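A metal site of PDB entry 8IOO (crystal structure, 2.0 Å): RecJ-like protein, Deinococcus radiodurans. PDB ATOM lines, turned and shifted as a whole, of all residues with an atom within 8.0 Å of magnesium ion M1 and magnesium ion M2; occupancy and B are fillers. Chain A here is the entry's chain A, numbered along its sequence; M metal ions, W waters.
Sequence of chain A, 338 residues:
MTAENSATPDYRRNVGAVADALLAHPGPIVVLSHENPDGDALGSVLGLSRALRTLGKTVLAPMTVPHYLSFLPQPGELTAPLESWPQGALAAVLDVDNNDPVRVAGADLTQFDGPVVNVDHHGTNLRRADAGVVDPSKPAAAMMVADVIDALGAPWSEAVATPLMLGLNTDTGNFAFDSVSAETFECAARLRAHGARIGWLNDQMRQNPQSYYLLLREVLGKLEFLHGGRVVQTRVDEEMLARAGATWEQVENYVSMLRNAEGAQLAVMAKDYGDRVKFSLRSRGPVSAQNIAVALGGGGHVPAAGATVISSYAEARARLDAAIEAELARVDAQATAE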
ATOM      1  N   SER A  33      25.117 -32.940 -10.986  1.00  0.00           N
ATOM      2  CA  SER A  33      24.559 -31.932 -10.112  1.00  0.00           C
ATOM      3  C   SER A  33      23.707 -32.647  -9.060  1.00  0.00           C
ATOM      4  O   SER A  33      23.802 -33.871  -8.876  1.00  0.00           O
ATOM      5  CB  SER A  33      23.766 -30.880 -10.924  1.00  0.00           C
ATOM      6  OG  SER A  33      23.574 -29.710 -10.104  1.00  0.00           O
ATOM      7  N   HIS A  34      22.854 -31.880  -8.377  1.00  0.00           N
ATOM      8  CA  HIS A  34      22.195 -32.375  -7.178  1.00  0.00           C
ATOM      9  C   HIS A  34      20.909 -33.126  -7.497  1.00  0.00           C
ATOM     10  O   HIS A  34      20.325 -32.958  -8.574  1.00  0.00           O
ATOM     11  CB  HIS A  34      21.941 -31.202  -6.179  1.00  0.00           C
ATOM     12  CG  HIS A  34      20.987 -30.141  -6.673  1.00  0.00           C
ATOM     13  ND1 HIS A  34      19.624 -30.309  -6.705  1.00  0.00           N
ATOM     14  CD2 HIS A  34      21.221 -28.880  -7.116  1.00  0.00           C
ATOM     15  CE1 HIS A  34      19.056 -29.215  -7.172  1.00  0.00           C
ATOM     16  NE2 HIS A  34      19.998 -28.328  -7.427  1.00  0.00           N
ATOM     17  N   GLU A  35      20.491 -33.985  -6.566  1.00  0.00           N
ATOM     18  CA  GLU A  35      19.201 -34.663  -6.726  1.00  0.00           C
ATOM     19  C   GLU A  35      18.058 -33.665  -6.711  1.00  0.00           C
ATOM     20  O   GLU A  35      18.145 -32.572  -6.128  1.00  0.00           O
ATOM     21  CB  GLU A  35      19.023 -35.730  -5.624  1.00  0.00           C
ATOM     22  CG  GLU A  35      18.529 -35.242  -4.294  1.00  0.00           C
ATOM     23  CD  GLU A  35      18.719 -36.310  -3.219  1.00  0.00           C
ATOM     24  OE1 GLU A  35      18.257 -37.469  -3.435  1.00  0.00           O
ATOM     25  OE2 GLU A  35      19.264 -35.985  -2.145  1.00  0.00           O
ATOM     26  N   ASN A  36      16.950 -34.064  -7.339  1.00  0.00           N
ATOM     27  CA  ASN A  36      15.855 -33.188  -7.737  1.00  0.00           C
ATOM     28  C   ASN A  36      16.411 -31.914  -8.354  1.00  0.00           C
ATOM     29  O   ASN A  36      16.276 -30.822  -7.778  1.00  0.00           O
ATOM     30  CB  ASN A  36      14.890 -32.873  -6.584  1.00  0.00           C
ATOM     31  CG  ASN A  36      14.479 -34.125  -5.829  1.00  0.00           C
ATOM     32  OD1 ASN A  36      13.779 -34.976  -6.373  1.00  0.00           O
ATOM     33  ND2 ASN A  36      14.894 -34.218  -4.575  1.00  0.00           N
ATOM     34  N   PRO A  37      17.017 -32.020  -9.525  1.00  0.00           N
ATOM     35  CA  PRO A  37      17.678 -30.867 -10.144  1.00  0.00           C
ATOM     36  C   PRO A  37      16.702 -29.719 -10.342  1.00  0.00           C
ATOM     37  O   PRO A  37      15.558 -29.924 -10.744  1.00  0.00           O
ATOM     38  CB  PRO A  37      18.135 -31.392 -11.512  1.00  0.00           C
ATOM     39  CG  PRO A  37      17.325 -32.671 -11.724  1.00  0.00           C
ATOM     40  CD  PRO A  37      17.130 -33.233 -10.372  1.00  0.00           C
ATOM     41  N   ASP A  38      17.185 -28.504 -10.168  1.00  0.00           N
ATOM     42  CA  ASP A  38      16.349 -27.318 -10.487  1.00  0.00           C
ATOM     43  C   ASP A  38      16.792 -26.783 -11.855  1.00  0.00           C
ATOM     44  O   ASP A  38      17.650 -27.413 -12.481  1.00  0.00           O
ATOM     45  CB  ASP A  38      16.452 -26.275  -9.374  1.00  0.00           C
ATOM     46  CG  ASP A  38      17.867 -25.975  -8.913  1.00  0.00           C
ATOM     47  OD1 ASP A  38      18.753 -25.871  -9.772  1.00  0.00           O
ATOM     48  OD2 ASP A  38      18.065 -25.851  -7.702  1.00  0.00           O
ATOM     49  N   GLY A  39      16.249 -25.649 -12.270  1.00  0.00           N
ATOM     50  CA  GLY A  39      16.633 -25.052 -13.558  1.00  0.00           C
ATOM     51  C   GLY A  39      18.116 -24.738 -13.612  1.00  0.00           C
ATOM     52  O   GLY A  39      18.705 -24.914 -14.679  1.00  0.00           O
ATOM     53  N   ASP A  40      18.689 -24.282 -12.508  1.00  0.00           N
ATOM     54  CA  ASP A  40      20.142 -23.963 -12.442  1.00  0.00           C
ATOM     55  C   ASP A  40      20.964 -25.236 -12.607  1.00  0.00           C
ATOM     56  O   ASP A  40      21.935 -25.204 -13.334  1.00  0.00           O
ATOM     57  CB  ASP A  40      20.481 -23.232 -11.135  1.00  0.00           C
ATOM     58  CG  ASP A  40      21.874 -22.644 -11.104  1.00  0.00           C
ATOM     59  OD1 ASP A  40      22.342 -22.188 -12.148  1.00  0.00           O
ATOM     60  OD2 ASP A  40      22.477 -22.662 -10.017  1.00  0.00           O
ATOM     61  N   ALA A  41      20.578 -26.315 -11.929  1.00  0.00           N
ATOM     62  CA  ALA A  41      21.285 -27.602 -12.043  1.00  0.00           C
ATOM     63  C   ALA A  41      21.235 -28.122 -13.485  1.00  0.00           C
ATOM     64  O   ALA A  41      22.297 -28.395 -14.046  1.00  0.00           O
ATOM     65  CB  ALA A  41      20.676 -28.615 -11.101  1.00  0.00           C
ATOM     66  N   LEU A  42      20.031 -28.249 -14.047  1.00  0.00           N
ATOM     67  CA  LEU A  42      19.870 -28.781 -15.420  1.00  0.00           C
ATOM     68  C   LEU A  42      20.539 -27.809 -16.393  1.00  0.00           C
ATOM     69  O   LEU A  42      21.305 -28.268 -17.223  1.00  0.00           O
ATOM     70  CB  LEU A  42      18.383 -28.932 -15.755  1.00  0.00           C
ATOM     71  CG  LEU A  42      18.067 -29.325 -17.198  1.00  0.00           C
ATOM     72  CD1 LEU A  42      18.661 -30.680 -17.536  1.00  0.00           C
ATOM     73  CD2 LEU A  42      16.572 -29.326 -17.444  1.00  0.00           C
ATOM     74  N   SER A  44      22.912 -25.592 -15.972  1.00  0.00           N
ATOM     75  CA  SER A  44      24.372 -25.630 -15.879  1.00  0.00           C
ATOM     76  C   SER A  44      24.931 -26.920 -16.454  1.00  0.00           C
ATOM     77  O   SER A  44      25.950 -26.903 -17.150  1.00  0.00           O
ATOM     78  CB  SER A  44      24.888 -25.450 -14.441  1.00  0.00           C
ATOM     79  OG  SER A  44      24.359 -24.306 -13.795  1.00  0.00           O
ATOM     80  N   LEU A  94      28.455 -29.664 -10.389  1.00  0.00           N
ATOM     81  CA  LEU A  94      27.957 -28.293 -10.511  1.00  0.00           C
ATOM     82  C   LEU A  94      26.774 -28.074  -9.573  1.00  0.00           C
ATOM     83  O   LEU A  94      25.924 -28.959  -9.424  1.00  0.00           O
ATOM     84  CB  LEU A  94      27.489 -28.002 -11.940  1.00  0.00           C
ATOM     85  CG  LEU A  94      28.410 -28.554 -13.025  1.00  0.00           C
ATOM     86  CD1 LEU A  94      27.794 -28.338 -14.410  1.00  0.00           C
ATOM     87  CD2 LEU A  94      29.851 -28.021 -12.938  1.00  0.00           C
ATOM     88  N   ASP A  95      26.704 -26.886  -8.972  1.00  0.00           N
ATOM     89  CA  ASP A  95      25.505 -26.402  -8.256  1.00  0.00           C
ATOM     90  C   ASP A  95      25.289 -27.210  -6.987  1.00  0.00           C
ATOM     91  O   ASP A  95      24.188 -27.228  -6.426  1.00  0.00           O
ATOM     92  CB  ASP A  95      24.246 -26.458  -9.143  1.00  0.00           C
ATOM     93  CG  ASP A  95      23.056 -25.608  -8.584  1.00  0.00           C
ATOM     94  OD1 ASP A  95      23.277 -24.439  -8.207  1.00  0.00           O
ATOM     95  OD2 ASP A  95      21.925 -26.112  -8.491  1.00  0.00           O
ATOM     96  N   VAL A  96      26.332 -27.905  -6.523  1.00  0.00           N
ATOM     97  CA  VAL A  96      26.271 -28.696  -5.294  1.00  0.00           C
ATOM     98  C   VAL A  96      27.720 -28.950  -4.905  1.00  0.00           C
ATOM     99  O   VAL A  96      28.639 -28.763  -5.709  1.00  0.00           O
ATOM    100  CB  VAL A  96      25.465 -30.010  -5.492  1.00  0.00           C
ATOM    101  CG1 VAL A  96      26.145 -30.891  -6.534  1.00  0.00           C
ATOM    102  CG2 VAL A  96      25.245 -30.775  -4.174  1.00  0.00           C
ATOM    103  N   VAL A 119      32.015 -26.483  -9.297  1.00  0.00           N
ATOM    104  CA  VAL A 119      31.550 -25.136  -9.610  1.00  0.00           C
ATOM    105  C   VAL A 119      30.257 -24.938  -8.820  1.00  0.00           C
ATOM    106  O   VAL A 119      29.241 -25.565  -9.135  1.00  0.00           O
ATOM    107  CB  VAL A 119      31.310 -24.921 -11.118  1.00  0.00           C
ATOM    108  CG1 VAL A 119      30.774 -23.502 -11.442  1.00  0.00           C
ATOM    109  CG2 VAL A 119      32.581 -25.221 -11.933  1.00  0.00           C
ATOM    110  N   ASP A 120      30.290 -24.078  -7.793  1.00  0.00           N
ATOM    111  CA  ASP A 120      29.143 -24.004  -6.880  1.00  0.00           C
ATOM    112  C   ASP A 120      28.984 -22.578  -6.355  1.00  0.00           C
ATOM    113  O   ASP A 120      29.924 -21.773  -6.373  1.00  0.00           O
ATOM    114  CB  ASP A 120      29.310 -25.008  -5.724  1.00  0.00           C
ATOM    115  CG  ASP A 120      28.019 -25.267  -4.957  1.00  0.00           C
ATOM    116  OD1 ASP A 120      26.939 -24.919  -5.466  1.00  0.00           O
ATOM    117  OD2 ASP A 120      28.112 -25.873  -3.857  1.00  0.00           O
ATOM    118  N   HIS A 121      27.778 -22.283  -5.866  1.00  0.00           N
ATOM    119  CA  HIS A 121      27.467 -20.955  -5.356  1.00  0.00           C
ATOM    120  C   HIS A 121      26.733 -20.994  -4.002  1.00  0.00           C
ATOM    121  O   HIS A 121      26.052 -20.028  -3.642  1.00  0.00           O
ATOM    122  CB  HIS A 121      26.676 -20.145  -6.410  1.00  0.00           C
ATOM    123  CG  HIS A 121      25.254 -20.594  -6.604  1.00  0.00           C
ATOM    124  ND1 HIS A 121      24.183 -19.741  -6.426  1.00  0.00           N
ATOM    125  CD2 HIS A 121      24.739 -21.779  -7.001  1.00  0.00           C
ATOM    126  CE1 HIS A 121      23.064 -20.398  -6.692  1.00  0.00           C
ATOM    127  NE2 HIS A 121      23.375 -21.638  -7.036  1.00  0.00           N
ATOM    128  N   HIS A 122      26.859 -22.075  -3.232  1.00  0.00           N
ATOM    129  CA  HIS A 122      26.359 -22.142  -1.860  1.00  0.00           C
ATOM    130  C   HIS A 122      27.491 -22.038  -0.854  1.00  0.00           C
ATOM    131  O   HIS A 122      28.560 -22.631  -1.029  1.00  0.00           O
ATOM    132  CB  HIS A 122      25.585 -23.429  -1.583  1.00  0.00           C
ATOM    133  CG  HIS A 122      24.570 -23.755  -2.624  1.00  0.00           C
ATOM    134  ND1 HIS A 122      24.872 -24.485  -3.757  1.00  0.00           N
ATOM    135  CD2 HIS A 122      23.223 -23.564  -2.648  1.00  0.00           C
ATOM    136  CE1 HIS A 122      23.768 -24.652  -4.463  1.00  0.00           C
ATOM    137  NE2 HIS A 122      22.755 -24.113  -3.809  1.00  0.00           N
ATOM    138  N   LYS A 138      27.568 -15.049  -6.367  1.00  0.00           N
ATOM    139  CA  LYS A 138      26.892 -15.271  -7.638  1.00  0.00           C
ATOM    140  C   LYS A 138      25.546 -15.922  -7.352  1.00  0.00           C
ATOM    141  O   LYS A 138      25.487 -16.902  -6.599  1.00  0.00           O
ATOM    142  CB  LYS A 138      27.744 -16.171  -8.555  1.00  0.00           C
ATOM    143  CG  LYS A 138      29.167 -15.653  -8.793  1.00  0.00           C
ATOM    144  CD  LYS A 138      29.268 -14.595  -9.875  1.00  0.00           C
ATOM    145  CE  LYS A 138      30.714 -14.368 -10.325  1.00  0.00           C
ATOM    146  NZ  LYS A 138      31.598 -13.970  -9.197  1.00  0.00           N
ATOM    147  N   PRO A 139      24.426 -15.405  -7.871  1.00  0.00           N
ATOM    148  CA  PRO A 139      23.128 -15.988  -7.521  1.00  0.00           C
ATOM    149  C   PRO A 139      22.756 -17.239  -8.308  1.00  0.00           C
ATOM    150  O   PRO A 139      21.687 -17.808  -8.058  1.00  0.00           O
ATOM    151  CB  PRO A 139      22.132 -14.856  -7.857  1.00  0.00           C
ATOM    152  CG  PRO A 139      22.763 -14.125  -8.992  1.00  0.00           C
ATOM    153  CD  PRO A 139      24.279 -14.265  -8.808  1.00  0.00           C
ATOM    154  N   ALA A 140      23.564 -17.671  -9.265  1.00  0.00           N
ATOM    155  CA  ALA A 140      23.232 -18.897  -9.992  1.00  0.00           C
ATOM    156  C   ALA A 140      24.516 -19.549 -10.441  1.00  0.00           C
ATOM    157  O   ALA A 140      25.427 -18.856 -10.925  1.00  0.00           O
ATOM    158  CB  ALA A 140      22.314 -18.617 -11.196  1.00  0.00           C
ATOM    159  N   ALA A 141      24.602 -20.865 -10.297  1.00  0.00           N
ATOM    160  CA  ALA A 141      25.785 -21.562 -10.800  1.00  0.00           C
ATOM    161  C   ALA A 141      25.928 -21.389 -12.303  1.00  0.00           C
ATOM    162  O   ALA A 141      27.057 -21.454 -12.809  1.00  0.00           O
ATOM    163  CB  ALA A 141      25.749 -23.056 -10.452  1.00  0.00           C
ATOM    164  N   ALA A 142      24.822 -21.132 -13.024  1.00  0.00           N
ATOM    165  CA  ALA A 142      24.913 -20.975 -14.481  1.00  0.00           C
ATOM    166  C   ALA A 142      25.786 -19.782 -14.876  1.00  0.00           C
ATOM    167  O   ALA A 142      26.507 -19.838 -15.895  1.00  0.00           O
ATOM    168  CB  ALA A 142      23.509 -20.859 -15.093  1.00  0.00           C
ATOM    169  N   GLY A 167      18.731 -21.349 -16.079  1.00  0.00           N
ATOM    170  CA  GLY A 167      19.268 -21.449 -14.708  1.00  0.00           C
ATOM    171  C   GLY A 167      19.346 -20.093 -14.058  1.00  0.00           C
ATOM    172  O   GLY A 167      18.960 -19.974 -12.900  1.00  0.00           O
ATOM    173  N   THR A 170      15.672 -19.115 -13.217  1.00  0.00           N
ATOM    174  CA  THR A 170      15.004 -19.857 -12.145  1.00  0.00           C
ATOM    175  C   THR A 170      15.667 -19.650 -10.787  1.00  0.00           C
ATOM    176  O   THR A 170      14.967 -19.591  -9.774  1.00  0.00           O
ATOM    177  CB  THR A 170      14.921 -21.349 -12.489  1.00  0.00           C
ATOM    178  OG1 THR A 170      16.230 -21.923 -12.559  1.00  0.00           O
ATOM    179  CG2 THR A 170      14.113 -21.579 -13.789  1.00  0.00           C
ATOM    180  N   ASP A 171      17.001 -19.554 -10.729  1.00  0.00           N
ATOM    181  CA  ASP A 171      17.651 -19.317  -9.423  1.00  0.00           C
ATOM    182  C   ASP A 171      17.498 -17.899  -8.899  1.00  0.00           C
ATOM    183  O   ASP A 171      17.703 -17.671  -7.701  1.00  0.00           O
ATOM    184  CB  ASP A 171      19.125 -19.682  -9.494  1.00  0.00           C
ATOM    185  CG  ASP A 171      19.435 -20.936  -8.760  1.00  0.00           C
ATOM    186  OD1 ASP A 171      18.538 -21.751  -8.514  1.00  0.00           O
ATOM    187  OD2 ASP A 171      20.640 -21.135  -8.515  1.00  0.00           O
ATOM    188  N   THR A 172      17.172 -16.934  -9.753  1.00  0.00           N
ATOM    189  CA  THR A 172      16.958 -15.569  -9.302  1.00  0.00           C
ATOM    190  C   THR A 172      15.491 -15.207  -9.294  1.00  0.00           C
ATOM    191  O   THR A 172      15.154 -14.040  -9.081  1.00  0.00           O
ATOM    192  CB  THR A 172      17.655 -14.556 -10.214  1.00  0.00           C
ATOM    193  OG1 THR A 172      17.139 -14.656 -11.547  1.00  0.00           O
ATOM    194  CG2 THR A 172      19.142 -14.754 -10.214  1.00  0.00           C
HETATM  195 MG    MG M   1      21.820 -22.951  -8.014  1.00  0.00          MG
HETATM  196 MG    MG M   2      20.479 -25.617  -7.675  1.00  0.00          MG
HETATM  197  O   HOH W   1      20.378 -25.704  -5.726  1.00  0.00           O
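Magnesium ion M1 is bound by OD1 of Asp 95 (2.1 Å).
OD2 of Asp 40 binds magnesium ion M1.
OD2 of Asp 171 is bound to magnesium ion M1, at 2.2 Å.
NE2 of His 121 binds magnesium ion M1 (2.3 Å).
Magnesium ion M1 has four donor atoms within binding distance.
OD2 of Asp 95 lies close to NE2 of His 34, at 3.1 Å.
N of Asp 95 sits at hydrogen-bond distance from O of Val 119.
N of Asp 40 is in hydrogen-bond range of OD1 of Asp 38 (3.2 Å).
The backbone NH (N) of Ala 141 sits at hydrogen-bond distance from the side-chain carboxylate (OD1) of Asp 40 (3.2 Å).
N of Ala 142 sits at hydrogen-bond distance from OD1 of Asp 40 (2.8 Å).
OG1 of Thr 170 sits at hydrogen-bond distance from N of Asp 40 (3.4 Å).
OD2 of Asp 38 lies close to NE2 of His 34 (3.2 Å).
The backbone NH (N) of Ala 41 lies within hydrogen-bond range of the side-chain carboxylate (OD1) of Asp 38 (2.9 Å).
Water W1 lies within hydrogen-bond range of NE2 of His 34 (3.2 Å) and NE2 of His 122 (3.4 Å).
Of the 27 residues printed, 4 come within 4 Å of magnesium ion M1.
Along chain A the residues within 4 Å of magnesium ion M1 span positions 40 to 171.
Magnesium ion M2 is bound by the side-chain carboxylate (OD2) of Asp 95 (1.7 Å).
Magnesium ion M2 is bound by water W1 (2.0 Å).
OD2 of Asp 38 binds magnesium ion M2 (2.4 Å).
Slightly farther from magnesium ion M2 lies the side-chain carboxylate (OD1) of Asp 38 (2.7 Å).
Slightly farther from magnesium ion M2 lies a ring nitrogen (NE2) of His 34 (2.8 Å).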
